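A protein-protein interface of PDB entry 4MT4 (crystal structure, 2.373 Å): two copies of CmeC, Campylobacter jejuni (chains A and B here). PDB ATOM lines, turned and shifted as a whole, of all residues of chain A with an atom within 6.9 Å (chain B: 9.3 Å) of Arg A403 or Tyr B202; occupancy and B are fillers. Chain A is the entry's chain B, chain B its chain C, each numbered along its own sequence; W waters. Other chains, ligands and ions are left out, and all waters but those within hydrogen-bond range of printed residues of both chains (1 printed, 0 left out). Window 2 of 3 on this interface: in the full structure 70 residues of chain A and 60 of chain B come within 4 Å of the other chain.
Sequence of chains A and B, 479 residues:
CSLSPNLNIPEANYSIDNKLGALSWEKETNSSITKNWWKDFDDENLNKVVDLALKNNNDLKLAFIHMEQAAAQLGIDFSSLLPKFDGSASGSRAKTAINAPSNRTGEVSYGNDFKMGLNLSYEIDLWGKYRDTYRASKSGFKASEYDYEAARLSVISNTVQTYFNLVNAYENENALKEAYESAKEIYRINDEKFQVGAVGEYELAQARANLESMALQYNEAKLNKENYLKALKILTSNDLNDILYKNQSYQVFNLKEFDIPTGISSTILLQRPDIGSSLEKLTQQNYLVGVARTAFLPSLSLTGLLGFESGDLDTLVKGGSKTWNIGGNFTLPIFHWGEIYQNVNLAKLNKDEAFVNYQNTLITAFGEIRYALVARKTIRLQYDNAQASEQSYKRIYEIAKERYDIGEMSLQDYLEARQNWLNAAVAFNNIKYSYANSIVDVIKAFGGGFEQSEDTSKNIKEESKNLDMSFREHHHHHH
The guanidinium group of Arg A395 lies within salt-bridge range of the side-chain carboxylate of Glu B201 (2.5 Å).
2 positions are printed for both chains. Of the 8 pairs that touch across the chains among the printed residues, none has its exchanged pair printed and touching as well.
Among the printed residues, pairs that only touch across the chains: Ile A396 with Tyr B202, Ile A399 with Tyr B202, Ile A396 with Ala B205, Ile A396 with Gln B206, Met A409 with Tyr B202, Arg A403 with Tyr B202 and Ile A396 with Ala B209.
Printed residues of chain B within 4 Å of Arg A395: Glu B201 (2.5 Å). Printed residues of chain B within 4 Å of Ile A399: Tyr B202. No residue of chain B comes within 4 Å of Ala A400. No residue of chain B comes within 4 Å of Gly A407. Met A409 touches one residue of chain B. Printed residues of chain A within 4 Å of Glu B201: Arg A395. Of chain A, only Ile A396 (3.6 Å), Ile A399 (3.6 Å), Arg A403 (3.9 Å) and Met A409 (3.8 Å) come within 4 Å of Tyr B202. Glu B203 touches none of the printed residues of chain A. Of the printed residues of chain A, Gln B206 touches Ile A396 (3.7 Å). Of the printed residues of chain A, Ala B209 touches Ile A396 (3.99 Å). The nearest residue of chain B that does not touch Arg A403 is Glu B203 (4.9 Å). The nearest printed residue of chain A that does not touch Glu B201 is Ile A399 (4.2 Å).
The side-chain carboxylate of Glu A398 is in salt-bridge range of the guanidinium group of Arg A395 (3.6 Å). The backbone NH (N) of Glu A408 is in hydrogen-bond range of the backbone carbonyl oxygen (O) of Arg A403 (2.7 Å). The backbone carbonyl oxygen (O) of Arg A403 sits at hydrogen-bond distance from the backbone NH (N) of Met A409, at 3.5 Å.
Water W1 lies within hydrogen-bond range of the guanidinium group of Arg A403 and the side-chain carboxylate of Glu B203.
Of the 18 printed residues of chain A, 5 touch a printed residue of chain B. Printed residues of chain B that touch a printed residue of chain A: Glu B201, Tyr B202, Ala B205, Gln B206 and Ala B209. Hydrophobic or aromatic side chains of chain B within 4 Å of the printed part of chain A: Tyr B202, Ala B205 and Ala B209. Among the printed residues, Asp or Glu carboxylates within 4 Å of a Lys or Arg side-chain nitrogen of the other chain: Arg A395 with Glu B201 (2.5 Å).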
ATOM      1  N   ARG A 395     -19.796  21.230  -5.470  1.00  0.00           N
ATOM      2  CA  ARG A 395     -21.057  20.500  -5.550  1.00  0.00           C
ATOM      3  C   ARG A 395     -22.209  21.381  -5.084  1.00  0.00           C
ATOM      4  O   ARG A 395     -23.302  21.333  -5.641  1.00  0.00           O
ATOM      5  CB  ARG A 395     -20.999  19.220  -4.715  1.00  0.00           C
ATOM      6  CG  ARG A 395     -22.274  18.385  -4.763  1.00  0.00           C
ATOM      7  CD  ARG A 395     -22.620  17.987  -6.189  1.00  0.00           C
ATOM      8  NE  ARG A 395     -23.856  17.214  -6.265  1.00  0.00           N
ATOM      9  CZ  ARG A 395     -24.827  17.440  -7.146  1.00  0.00           C
ATOM     10  NH1 ARG A 395     -24.710  18.422  -8.030  1.00  0.00           N
ATOM     11  NH2 ARG A 395     -25.917  16.684  -7.144  1.00  0.00           N
ATOM     12  N   ILE A 396     -21.951  22.180  -4.052  1.00  0.00           N
ATOM     13  CA  ILE A 396     -22.922  23.151  -3.562  1.00  0.00           C
ATOM     14  C   ILE A 396     -23.289  24.143  -4.662  1.00  0.00           C
ATOM     15  O   ILE A 396     -24.460  24.469  -4.853  1.00  0.00           O
ATOM     16  CB  ILE A 396     -22.385  23.917  -2.335  1.00  0.00           C
ATOM     17  CG1 ILE A 396     -22.259  22.980  -1.131  1.00  0.00           C
ATOM     18  CG2 ILE A 396     -23.294  25.089  -1.996  1.00  0.00           C
ATOM     19  CD1 ILE A 396     -21.604  23.617   0.075  1.00  0.00           C
ATOM     20  N   TYR A 397     -22.277  24.608  -5.388  1.00  0.00           N
ATOM     21  CA  TYR A 397     -22.488  25.533  -6.495  1.00  0.00           C
ATOM     22  C   TYR A 397     -23.287  24.892  -7.625  1.00  0.00           C
ATOM     23  O   TYR A 397     -24.169  25.523  -8.205  1.00  0.00           O
ATOM     24  CB  TYR A 397     -21.154  26.042  -7.041  1.00  0.00           C
ATOM     25  CG  TYR A 397     -21.284  26.686  -8.404  1.00  0.00           C
ATOM     26  CD1 TYR A 397     -21.840  27.952  -8.543  1.00  0.00           C
ATOM     27  CD2 TYR A 397     -20.862  26.026  -9.552  1.00  0.00           C
ATOM     28  CE1 TYR A 397     -21.969  28.543  -9.784  1.00  0.00           C
ATOM     29  CE2 TYR A 397     -20.989  26.609 -10.798  1.00  0.00           C
ATOM     30  CZ  TYR A 397     -21.542  27.868 -10.909  1.00  0.00           C
ATOM     31  OH  TYR A 397     -21.668  28.455 -12.148  1.00  0.00           O
ATOM     32  N   GLU A 398     -22.964  23.640  -7.939  1.00  0.00           N
ATOM     33  CA  GLU A 398     -23.634  22.927  -9.021  1.00  0.00           C
ATOM     34  C   GLU A 398     -25.126  22.780  -8.749  1.00  0.00           C
ATOM     35  O   GLU A 398     -25.944  22.911  -9.658  1.00  0.00           O
ATOM     36  CB  GLU A 398     -22.999  21.550  -9.232  1.00  0.00           C
ATOM     37  CG  GLU A 398     -21.606  21.600  -9.840  1.00  0.00           C
ATOM     38  CD  GLU A 398     -20.980  20.226  -9.969  1.00  0.00           C
ATOM     39  OE1 GLU A 398     -21.431  19.301  -9.262  1.00  0.00           O
ATOM     40  OE2 GLU A 398     -20.042  20.069 -10.779  1.00  0.00           O
ATOM     41  N   ILE A 399     -25.475  22.518  -7.495  1.00  0.00           N
ATOM     42  CA  ILE A 399     -26.875  22.416  -7.103  1.00  0.00           C
ATOM     43  C   ILE A 399     -27.526  23.796  -7.090  1.00  0.00           C
ATOM     44  O   ILE A 399     -28.672  23.958  -7.509  1.00  0.00           O
ATOM     45  CB  ILE A 399     -27.030  21.763  -5.715  1.00  0.00           C
ATOM     46  CG1 ILE A 399     -26.384  20.379  -5.699  1.00  0.00           C
ATOM     47  CG2 ILE A 399     -28.498  21.658  -5.331  1.00  0.00           C
ATOM     48  CD1 ILE A 399     -26.431  19.701  -4.346  1.00  0.00           C
ATOM     49  N   ALA A 400     -26.782  24.791  -6.618  1.00  0.00           N
ATOM     50  CA  ALA A 400     -27.293  26.155  -6.512  1.00  0.00           C
ATOM     51  C   ALA A 400     -27.574  26.759  -7.884  1.00  0.00           C
ATOM     52  O   ALA A 400     -28.453  27.610  -8.026  1.00  0.00           O
ATOM     53  CB  ALA A 400     -26.315  27.029  -5.741  1.00  0.00           C
ATOM     54  N   LYS A 401     -26.827  26.323  -8.892  1.00  0.00           N
ATOM     55  CA  LYS A 401     -27.035  26.810 -10.251  1.00  0.00           C
ATOM     56  C   LYS A 401     -28.306  26.218 -10.850  1.00  0.00           C
ATOM     57  O   LYS A 401     -29.062  26.910 -11.531  1.00  0.00           O
ATOM     58  CB  LYS A 401     -25.834  26.481 -11.142  1.00  0.00           C
ATOM     59  CG  LYS A 401     -26.046  26.842 -12.606  1.00  0.00           C
ATOM     60  CD  LYS A 401     -24.814  26.564 -13.447  1.00  0.00           C
ATOM     61  CE  LYS A 401     -25.130  26.681 -14.931  1.00  0.00           C
ATOM     62  NZ  LYS A 401     -25.779  27.980 -15.259  1.00  0.00           N
ATOM     63  N   GLU A 402     -28.531  24.933 -10.591  1.00  0.00           N
ATOM     64  CA  GLU A 402     -29.731  24.246 -11.054  1.00  0.00           C
ATOM     65  C   GLU A 402     -30.991  24.894 -10.488  1.00  0.00           C
ATOM     66  O   GLU A 402     -31.989  25.057 -11.191  1.00  0.00           O
ATOM     67  CB  GLU A 402     -29.685  22.765 -10.661  1.00  0.00           C
ATOM     68  CG  GLU A 402     -28.565  21.975 -11.318  1.00  0.00           C
ATOM     69  CD  GLU A 402     -28.407  20.584 -10.730  1.00  0.00           C
ATOM     70  OE1 GLU A 402     -28.989  20.319  -9.657  1.00  0.00           O
ATOM     71  OE2 GLU A 402     -27.700  19.756 -11.342  1.00  0.00           O
ATOM     72  N   ARG A 403     -30.928  25.267  -9.214  1.00  0.00           N
ATOM     73  CA  ARG A 403     -32.066  25.860  -8.522  1.00  0.00           C
ATOM     74  C   ARG A 403     -32.324  27.293  -8.971  1.00  0.00           C
ATOM     75  O   ARG A 403     -33.475  27.718  -9.084  1.00  0.00           O
ATOM     76  CB  ARG A 403     -31.848  25.816  -7.008  1.00  0.00           C
ATOM     77  CG  ARG A 403     -31.759  24.409  -6.439  1.00  0.00           C
ATOM     78  CD  ARG A 403     -31.653  24.426  -4.920  1.00  0.00           C
ATOM     79  NE  ARG A 403     -31.716  23.079  -4.360  1.00  0.00           N
ATOM     80  CZ  ARG A 403     -31.691  22.808  -3.058  1.00  0.00           C
ATOM     81  NH1 ARG A 403     -31.603  23.791  -2.174  1.00  0.00           N
ATOM     82  NH2 ARG A 403     -31.754  21.550  -2.642  1.00  0.00           N
ATOM     83  N   TYR A 404     -31.254  28.040  -9.222  1.00  0.00           N
ATOM     84  CA  TYR A 404     -31.386  29.417  -9.679  1.00  0.00           C
ATOM     85  C   TYR A 404     -31.992  29.480 -11.076  1.00  0.00           C
ATOM     86  O   TYR A 404     -32.751  30.394 -11.392  1.00  0.00           O
ATOM     87  CB  TYR A 404     -30.031  30.129  -9.667  1.00  0.00           C
ATOM     88  CG  TYR A 404     -30.055  31.479 -10.352  1.00  0.00           C
ATOM     89  CD1 TYR A 404     -30.531  32.605  -9.695  1.00  0.00           C
ATOM     90  CD2 TYR A 404     -29.605  31.625 -11.660  1.00  0.00           C
ATOM     91  CE1 TYR A 404     -30.560  33.838 -10.320  1.00  0.00           C
ATOM     92  CE2 TYR A 404     -29.632  32.853 -12.291  1.00  0.00           C
ATOM     93  CZ  TYR A 404     -30.109  33.956 -11.617  1.00  0.00           C
ATOM     94  OH  TYR A 404     -30.136  35.184 -12.240  1.00  0.00           O
ATOM     95  N   ASP A 405     -31.654  28.504 -11.912  1.00  0.00           N
ATOM     96  CA  ASP A 405     -32.115  28.498 -13.295  1.00  0.00           C
ATOM     97  C   ASP A 405     -33.618  28.247 -13.402  1.00  0.00           C
ATOM     98  O   ASP A 405     -34.251  28.662 -14.371  1.00  0.00           O
ATOM     99  CB  ASP A 405     -31.347  27.454 -14.108  1.00  0.00           C
ATOM    100  CG  ASP A 405     -29.903  27.854 -14.352  1.00  0.00           C
ATOM    101  OD1 ASP A 405     -29.605  29.065 -14.294  1.00  0.00           O
ATOM    102  OD2 ASP A 405     -29.069  26.960 -14.606  1.00  0.00           O
ATOM    103  N   ILE A 406     -34.191  27.576 -12.407  1.00  0.00           N
ATOM    104  CA  ILE A 406     -35.628  27.334 -12.400  1.00  0.00           C
ATOM    105  C   ILE A 406     -36.324  28.251 -11.398  1.00  0.00           C
ATOM    106  O   ILE A 406     -37.504  28.073 -11.091  1.00  0.00           O
ATOM    107  CB  ILE A 406     -35.959  25.862 -12.083  1.00  0.00           C
ATOM    108  CG1 ILE A 406     -35.494  25.489 -10.675  1.00  0.00           C
ATOM    109  CG2 ILE A 406     -35.328  24.938 -13.116  1.00  0.00           C
ATOM    110  CD1 ILE A 406     -35.819  24.060 -10.293  1.00  0.00           C
ATOM    111  N   GLY A 407     -35.584  29.237 -10.897  1.00  0.00           N
ATOM    112  CA  GLY A 407     -36.155  30.270 -10.051  1.00  0.00           C
ATOM    113  C   GLY A 407     -36.385  29.872  -8.607  1.00  0.00           C
ATOM    114  O   GLY A 407     -37.119  30.546  -7.886  1.00  0.00           O
ATOM    115  N   GLU A 408     -35.756  28.782  -8.179  1.00  0.00           N
ATOM    116  CA  GLU A 408     -35.934  28.285  -6.820  1.00  0.00           C
ATOM    117  C   GLU A 408     -34.813  28.742  -5.888  1.00  0.00           C
ATOM    118  O   GLU A 408     -34.633  28.192  -4.801  1.00  0.00           O
ATOM    119  CB  GLU A 408     -36.030  26.758  -6.822  1.00  0.00           C
ATOM    120  CG  GLU A 408     -37.307  26.229  -7.455  1.00  0.00           C
ATOM    121  CD  GLU A 408     -37.449  24.727  -7.314  1.00  0.00           C
ATOM    122  OE1 GLU A 408     -36.466  24.075  -6.906  1.00  0.00           O
ATOM    123  OE2 GLU A 408     -38.544  24.200  -7.609  1.00  0.00           O
ATOM    124  N   MET A 409     -34.066  29.752  -6.321  1.00  0.00           N
ATOM    125  CA  MET A 409     -33.043  30.365  -5.483  1.00  0.00           C
ATOM    126  C   MET A 409     -32.795  31.807  -5.912  1.00  0.00           C
ATOM    127  O   MET A 409     -32.710  32.104  -7.103  1.00  0.00           O
ATOM    128  CB  MET A 409     -31.739  29.563  -5.534  1.00  0.00           C
ATOM    129  CG  MET A 409     -30.612  30.178  -4.711  1.00  0.00           C
ATOM    130  SD  MET A 409     -29.105  29.186  -4.669  1.00  0.00           S
ATOM    131  CE  MET A 409     -29.669  27.741  -3.772  1.00  0.00           C
ATOM    132  N   SER A 410     -32.684  32.700  -4.934  1.00  0.00           N
ATOM    133  CA  SER A 410     -32.417  34.106  -5.204  1.00  0.00           C
ATOM    134  C   SER A 410     -31.049  34.282  -5.853  1.00  0.00           C
ATOM    135  O   SER A 410     -30.153  33.457  -5.665  1.00  0.00           O
ATOM    136  CB  SER A 410     -32.493  34.925  -3.914  1.00  0.00           C
ATOM    137  OG  SER A 410     -31.458  34.554  -3.019  1.00  0.00           O
ATOM    138  N   ASP A 413     -28.187  34.531  -3.207  1.00  0.00           N
ATOM    139  CA  ASP A 413     -27.743  33.240  -2.695  1.00  0.00           C
ATOM    140  C   ASP A 413     -26.915  32.487  -3.732  1.00  0.00           C
ATOM    141  O   ASP A 413     -25.990  31.753  -3.387  1.00  0.00           O
ATOM    142  CB  ASP A 413     -28.941  32.388  -2.265  1.00  0.00           C
ATOM    143  CG  ASP A 413     -29.462  32.763  -0.891  1.00  0.00           C
ATOM    144  OD1 ASP A 413     -29.124  33.861  -0.402  1.00  0.00           O
ATOM    145  OD2 ASP A 413     -30.213  31.958  -0.300  1.00  0.00           O
ATOM    146  N   ALA A 417     -22.856  31.412  -3.360  1.00  0.00           N
ATOM    147  CA  ALA A 417     -22.402  30.032  -3.485  1.00  0.00           C
ATOM    148  C   ALA A 417     -21.274  29.924  -4.505  1.00  0.00           C
ATOM    149  O   ALA A 417     -20.339  29.139  -4.337  1.00  0.00           O
ATOM    150  CB  ALA A 417     -23.562  29.126  -3.874  1.00  0.00           C
ATOM    151  N   ASN B 190     -25.546  15.097  10.297  1.00  0.00           N
ATOM    152  CA  ASN B 190     -26.086  15.221   8.949  1.00  0.00           C
ATOM    153  C   ASN B 190     -25.790  13.995   8.091  1.00  0.00           C
ATOM    154  O   ASN B 190     -26.590  13.625   7.234  1.00  0.00           O
ATOM    155  CB  ASN B 190     -25.539  16.478   8.271  1.00  0.00           C
ATOM    156  CG  ASN B 190     -26.166  17.750   8.807  1.00  0.00           C
ATOM    157  OD1 ASN B 190     -27.102  18.289   8.217  1.00  0.00           O
ATOM    158  ND2 ASN B 190     -25.655  18.233   9.935  1.00  0.00           N
ATOM    159  N   PHE B 194     -28.671  11.766   6.511  1.00  0.00           N
ATOM    160  CA  PHE B 194     -28.674  11.646   5.056  1.00  0.00           C
ATOM    161  C   PHE B 194     -28.983  10.226   4.595  1.00  0.00           C
ATOM    162  O   PHE B 194     -29.723  10.023   3.635  1.00  0.00           O
ATOM    163  CB  PHE B 194     -27.328  12.089   4.478  1.00  0.00           C
ATOM    164  CG  PHE B 194     -27.193  11.830   3.006  1.00  0.00           C
ATOM    165  CD1 PHE B 194     -27.803  12.665   2.086  1.00  0.00           C
ATOM    166  CD2 PHE B 194     -26.463  10.747   2.542  1.00  0.00           C
ATOM    167  CE1 PHE B 194     -27.688  12.429   0.731  1.00  0.00           C
ATOM    168  CE2 PHE B 194     -26.344  10.504   1.187  1.00  0.00           C
ATOM    169  CZ  PHE B 194     -26.957  11.347   0.280  1.00  0.00           C
ATOM    170  N   VAL B 199     -31.954  14.396   5.610  1.00  0.00           N
ATOM    171  CA  VAL B 199     -31.387  15.621   5.048  1.00  0.00           C
ATOM    172  C   VAL B 199     -30.957  15.388   3.602  1.00  0.00           C
ATOM    173  O   VAL B 199     -30.711  14.254   3.194  1.00  0.00           O
ATOM    174  CB  VAL B 199     -30.175  16.138   5.861  1.00  0.00           C
ATOM    175  CG1 VAL B 199     -30.581  16.493   7.286  1.00  0.00           C
ATOM    176  CG2 VAL B 199     -29.051  15.124   5.856  1.00  0.00           C
ATOM    177  N   GLY B 200     -30.873  16.467   2.831  1.00  0.00           N
ATOM    178  CA  GLY B 200     -30.532  16.372   1.423  1.00  0.00           C
ATOM    179  C   GLY B 200     -29.041  16.457   1.156  1.00  0.00           C
ATOM    180  O   GLY B 200     -28.252  16.711   2.065  1.00  0.00           O
ATOM    181  N   GLU B 201     -28.662  16.237  -0.099  1.00  0.00           N
ATOM    182  CA  GLU B 201     -27.265  16.298  -0.513  1.00  0.00           C
ATOM    183  C   GLU B 201     -26.711  17.704  -0.342  1.00  0.00           C
ATOM    184  O   GLU B 201     -25.543  17.886  -0.001  1.00  0.00           O
ATOM    185  CB  GLU B 201     -27.119  15.852  -1.970  1.00  0.00           C
ATOM    186  CG  GLU B 201     -25.703  15.936  -2.524  1.00  0.00           C
ATOM    187  CD  GLU B 201     -25.640  15.635  -4.010  1.00  0.00           C
ATOM    188  OE1 GLU B 201     -26.711  15.470  -4.633  1.00  0.00           O
ATOM    189  OE2 GLU B 201     -24.520  15.561  -4.556  1.00  0.00           O
ATOM    190  N   TYR B 202     -27.563  18.696  -0.580  1.00  0.00           N
ATOM    191  CA  TYR B 202     -27.171  20.095  -0.469  1.00  0.00           C
ATOM    192  C   TYR B 202     -26.750  20.452   0.955  1.00  0.00           C
ATOM    193  O   TYR B 202     -25.735  21.117   1.161  1.00  0.00           O
ATOM    194  CB  TYR B 202     -28.319  21.000  -0.921  1.00  0.00           C
ATOM    195  CG  TYR B 202     -27.943  22.460  -1.044  1.00  0.00           C
ATOM    196  CD1 TYR B 202     -27.281  22.932  -2.170  1.00  0.00           C
ATOM    197  CD2 TYR B 202     -28.260  23.368  -0.041  1.00  0.00           C
ATOM    198  CE1 TYR B 202     -26.939  24.265  -2.293  1.00  0.00           C
ATOM    199  CE2 TYR B 202     -27.922  24.702  -0.153  1.00  0.00           C
ATOM    200  CZ  TYR B 202     -27.263  25.146  -1.282  1.00  0.00           C
ATOM    201  OH  TYR B 202     -26.925  26.474  -1.398  1.00  0.00           O
ATOM    202  N   GLU B 203     -27.530  20.004   1.933  1.00  0.00           N
ATOM    203  CA  GLU B 203     -27.218  20.268   3.334  1.00  0.00           C
ATOM    204  C   GLU B 203     -25.998  19.473   3.797  1.00  0.00           C
ATOM    205  O   GLU B 203     -25.170  19.979   4.553  1.00  0.00           O
ATOM    206  CB  GLU B 203     -28.420  19.947   4.225  1.00  0.00           C
ATOM    207  CG  GLU B 203     -29.585  20.919   4.080  1.00  0.00           C
ATOM    208  CD  GLU B 203     -30.439  20.638   2.860  1.00  0.00           C
ATOM    209  OE1 GLU B 203     -30.673  19.450   2.553  1.00  0.00           O
ATOM    210  OE2 GLU B 203     -30.874  21.610   2.206  1.00  0.00           O
ATOM    211  N   LEU B 204     -25.893  18.230   3.341  1.00  0.00           N
ATOM    212  CA  LEU B 204     -24.756  17.385   3.687  1.00  0.00           C
ATOM    213  C   LEU B 204     -23.457  17.984   3.158  1.00  0.00           C
ATOM    214  O   LEU B 204     -22.428  17.960   3.835  1.00  0.00           O
ATOM    215  CB  LEU B 204     -24.939  15.970   3.134  1.00  0.00           C
ATOM    216  CG  LEU B 204     -23.794  14.999   3.435  1.00  0.00           C
ATOM    217  CD1 LEU B 204     -23.662  14.774   4.934  1.00  0.00           C
ATOM    218  CD2 LEU B 204     -23.981  13.679   2.701  1.00  0.00           C
ATOM    219  N   ALA B 205     -23.516  18.524   1.945  1.00  0.00           N
ATOM    220  CA  ALA B 205     -22.359  19.154   1.323  1.00  0.00           C
ATOM    221  C   ALA B 205     -21.937  20.394   2.102  1.00  0.00           C
ATOM    222  O   ALA B 205     -20.748  20.665   2.258  1.00  0.00           O
ATOM    223  CB  ALA B 205     -22.662  19.510  -0.123  1.00  0.00           C
ATOM    224  N   GLN B 206     -22.923  21.143   2.589  1.00  0.00           N
ATOM    225  CA  GLN B 206     -22.666  22.325   3.404  1.00  0.00           C
ATOM    226  C   GLN B 206     -22.026  21.942   4.733  1.00  0.00           C
ATOM    227  O   GLN B 206     -21.178  22.663   5.259  1.00  0.00           O
ATOM    228  CB  GLN B 206     -23.960  23.102   3.650  1.00  0.00           C
ATOM    229  CG  GLN B 206     -24.465  23.878   2.445  1.00  0.00           C
ATOM    230  CD  GLN B 206     -25.797  24.557   2.704  1.00  0.00           C
ATOM    231  OE1 GLN B 206     -26.712  23.959   3.267  1.00  0.00           O
ATOM    232  NE2 GLN B 206     -25.908  25.815   2.295  1.00  0.00           N
ATOM    233  N   ALA B 207     -22.440  20.800   5.271  1.00  0.00           N
ATOM    234  CA  ALA B 207     -21.880  20.288   6.513  1.00  0.00           C
ATOM    235  C   ALA B 207     -20.436  19.840   6.309  1.00  0.00           C
ATOM    236  O   ALA B 207     -19.581  20.056   7.170  1.00  0.00           O
ATOM    237  CB  ALA B 207     -22.720  19.136   7.044  1.00  0.00           C
ATOM    238  N   ARG B 208     -20.168  19.222   5.163  1.00  0.00           N
ATOM    239  CA  ARG B 208     -18.824  18.754   4.851  1.00  0.00           C
ATOM    240  C   ARG B 208     -17.902  19.919   4.517  1.00  0.00           C
ATOM    241  O   ARG B 208     -16.747  19.948   4.941  1.00  0.00           O
ATOM    242  CB  ARG B 208     -18.847  17.758   3.691  1.00  0.00           C
ATOM    243  CG  ARG B 208     -17.469  17.239   3.320  1.00  0.00           C
ATOM    244  CD  ARG B 208     -17.490  15.754   2.995  1.00  0.00           C
ATOM    245  NE  ARG B 208     -16.235  15.111   3.374  1.00  0.00           N
ATOM    246  CZ  ARG B 208     -15.161  15.046   2.593  1.00  0.00           C
ATOM    247  NH1 ARG B 208     -15.185  15.585   1.382  1.00  0.00           N
ATOM    248  NH2 ARG B 208     -14.062  14.441   3.024  1.00  0.00           N
ATOM    249  N   ALA B 209     -18.421  20.877   3.753  1.00  0.00           N
ATOM    250  CA  ALA B 209     -17.662  22.068   3.386  1.00  0.00           C
ATOM    251  C   ALA B 209     -17.223  22.830   4.627  1.00  0.00           C
ATOM    252  O   ALA B 209     -16.078  23.267   4.728  1.00  0.00           O
ATOM    253  CB  ALA B 209     -18.488  22.967   2.479  1.00  0.00           C
ATOM    254  N   ASN B 210     -18.145  22.978   5.571  1.00  0.00           N
ATOM    255  CA  ASN B 210     -17.858  23.649   6.833  1.00  0.00           C
ATOM    256  C   ASN B 210     -16.845  22.872   7.667  1.00  0.00           C
ATOM    257  O   ASN B 210     -16.045  23.458   8.392  1.00  0.00           O
ATOM    258  CB  ASN B 210     -19.152  23.852   7.626  1.00  0.00           C
ATOM    259  CG  ASN B 210     -18.911  24.457   8.992  1.00  0.00           C
ATOM    260  OD1 ASN B 210     -18.776  25.673   9.132  1.00  0.00           O
ATOM    261  ND2 ASN B 210     -18.859  23.609  10.012  1.00  0.00           N
ATOM    262  N   SER B 410     -32.327  27.443   9.032  1.00  0.00           N
ATOM    263  CA  SER B 410     -31.602  26.667   8.036  1.00  0.00           C
ATOM    264  C   SER B 410     -30.200  26.322   8.528  1.00  0.00           C
ATOM    265  O   SER B 410     -29.675  26.968   9.438  1.00  0.00           O
ATOM    266  CB  SER B 410     -31.522  27.431   6.715  1.00  0.00           C
ATOM    267  OG  SER B 410     -30.747  28.607   6.858  1.00  0.00           O
ATOM    268  N   LEU B 411     -29.603  25.300   7.924  1.00  0.00           N
ATOM    269  CA  LEU B 411     -28.285  24.830   8.333  1.00  0.00           C
ATOM    270  C   LEU B 411     -27.203  25.889   8.142  1.00  0.00           C
ATOM    271  O   LEU B 411     -26.371  26.097   9.023  1.00  0.00           O
ATOM    272  CB  LEU B 411     -27.909  23.566   7.559  1.00  0.00           C
ATOM    273  CG  LEU B 411     -26.505  23.016   7.814  1.00  0.00           C
ATOM    274  CD1 LEU B 411     -26.344  22.576   9.262  1.00  0.00           C
ATOM    275  CD2 LEU B 411     -26.195  21.871   6.866  1.00  0.00           C
ATOM    276  N   GLN B 412     -27.221  26.563   6.994  1.00  0.00           N
ATOM    277  CA  GLN B 412     -26.154  27.500   6.649  1.00  0.00           C
ATOM    278  C   GLN B 412     -26.276  28.820   7.404  1.00  0.00           C
ATOM    279  O   GLN B 412     -25.294  29.546   7.555  1.00  0.00           O
ATOM    280  CB  GLN B 412     -26.127  27.760   5.139  1.00  0.00           C
ATOM    281  CG  GLN B 412     -27.170  28.740   4.631  1.00  0.00           C
ATOM    282  CD  GLN B 412     -26.888  29.192   3.209  1.00  0.00           C
ATOM    283  OE1 GLN B 412     -25.749  29.502   2.860  1.00  0.00           O
ATOM    284  NE2 GLN B 412     -27.923  29.219   2.378  1.00  0.00           N
ATOM    285  N   ASP B 413     -27.481  29.130   7.876  1.00  0.00           N
ATOM    286  CA  ASP B 413     -27.671  30.287   8.740  1.00  0.00           C
ATOM    287  C   ASP B 413     -27.121  29.979  10.127  1.00  0.00           C
ATOM    288  O   ASP B 413     -26.684  30.873  10.850  1.00  0.00           O
ATOM    289  CB  ASP B 413     -29.148  30.678   8.826  1.00  0.00           C
ATOM    290  CG  ASP B 413     -29.642  31.368   7.570  1.00  0.00           C
ATOM    291  OD1 ASP B 413     -28.808  31.940   6.835  1.00  0.00           O
ATOM    292  OD2 ASP B 413     -30.867  31.344   7.320  1.00  0.00           O
ATOM    293  N   LEU B 415     -24.571  27.691  10.546  1.00  0.00           N
ATOM    294  CA  LEU B 415     -23.132  27.581  10.341  1.00  0.00           C
ATOM    295  C   LEU B 415     -22.484  28.961  10.256  1.00  0.00           C
ATOM    296  O   LEU B 415     -21.371  29.165  10.740  1.00  0.00           O
ATOM    297  CB  LEU B 415     -22.828  26.776   9.075  1.00  0.00           C
ATOM    298  CG  LEU B 415     -23.250  25.306   9.099  1.00  0.00           C
ATOM    299  CD1 LEU B 415     -22.965  24.645   7.760  1.00  0.00           C
ATOM    300  CD2 LEU B 415     -22.550  24.563  10.227  1.00  0.00           C
HETATM  301  O   HOH W   1     -31.956  23.584   0.436  1.00  0.00           O
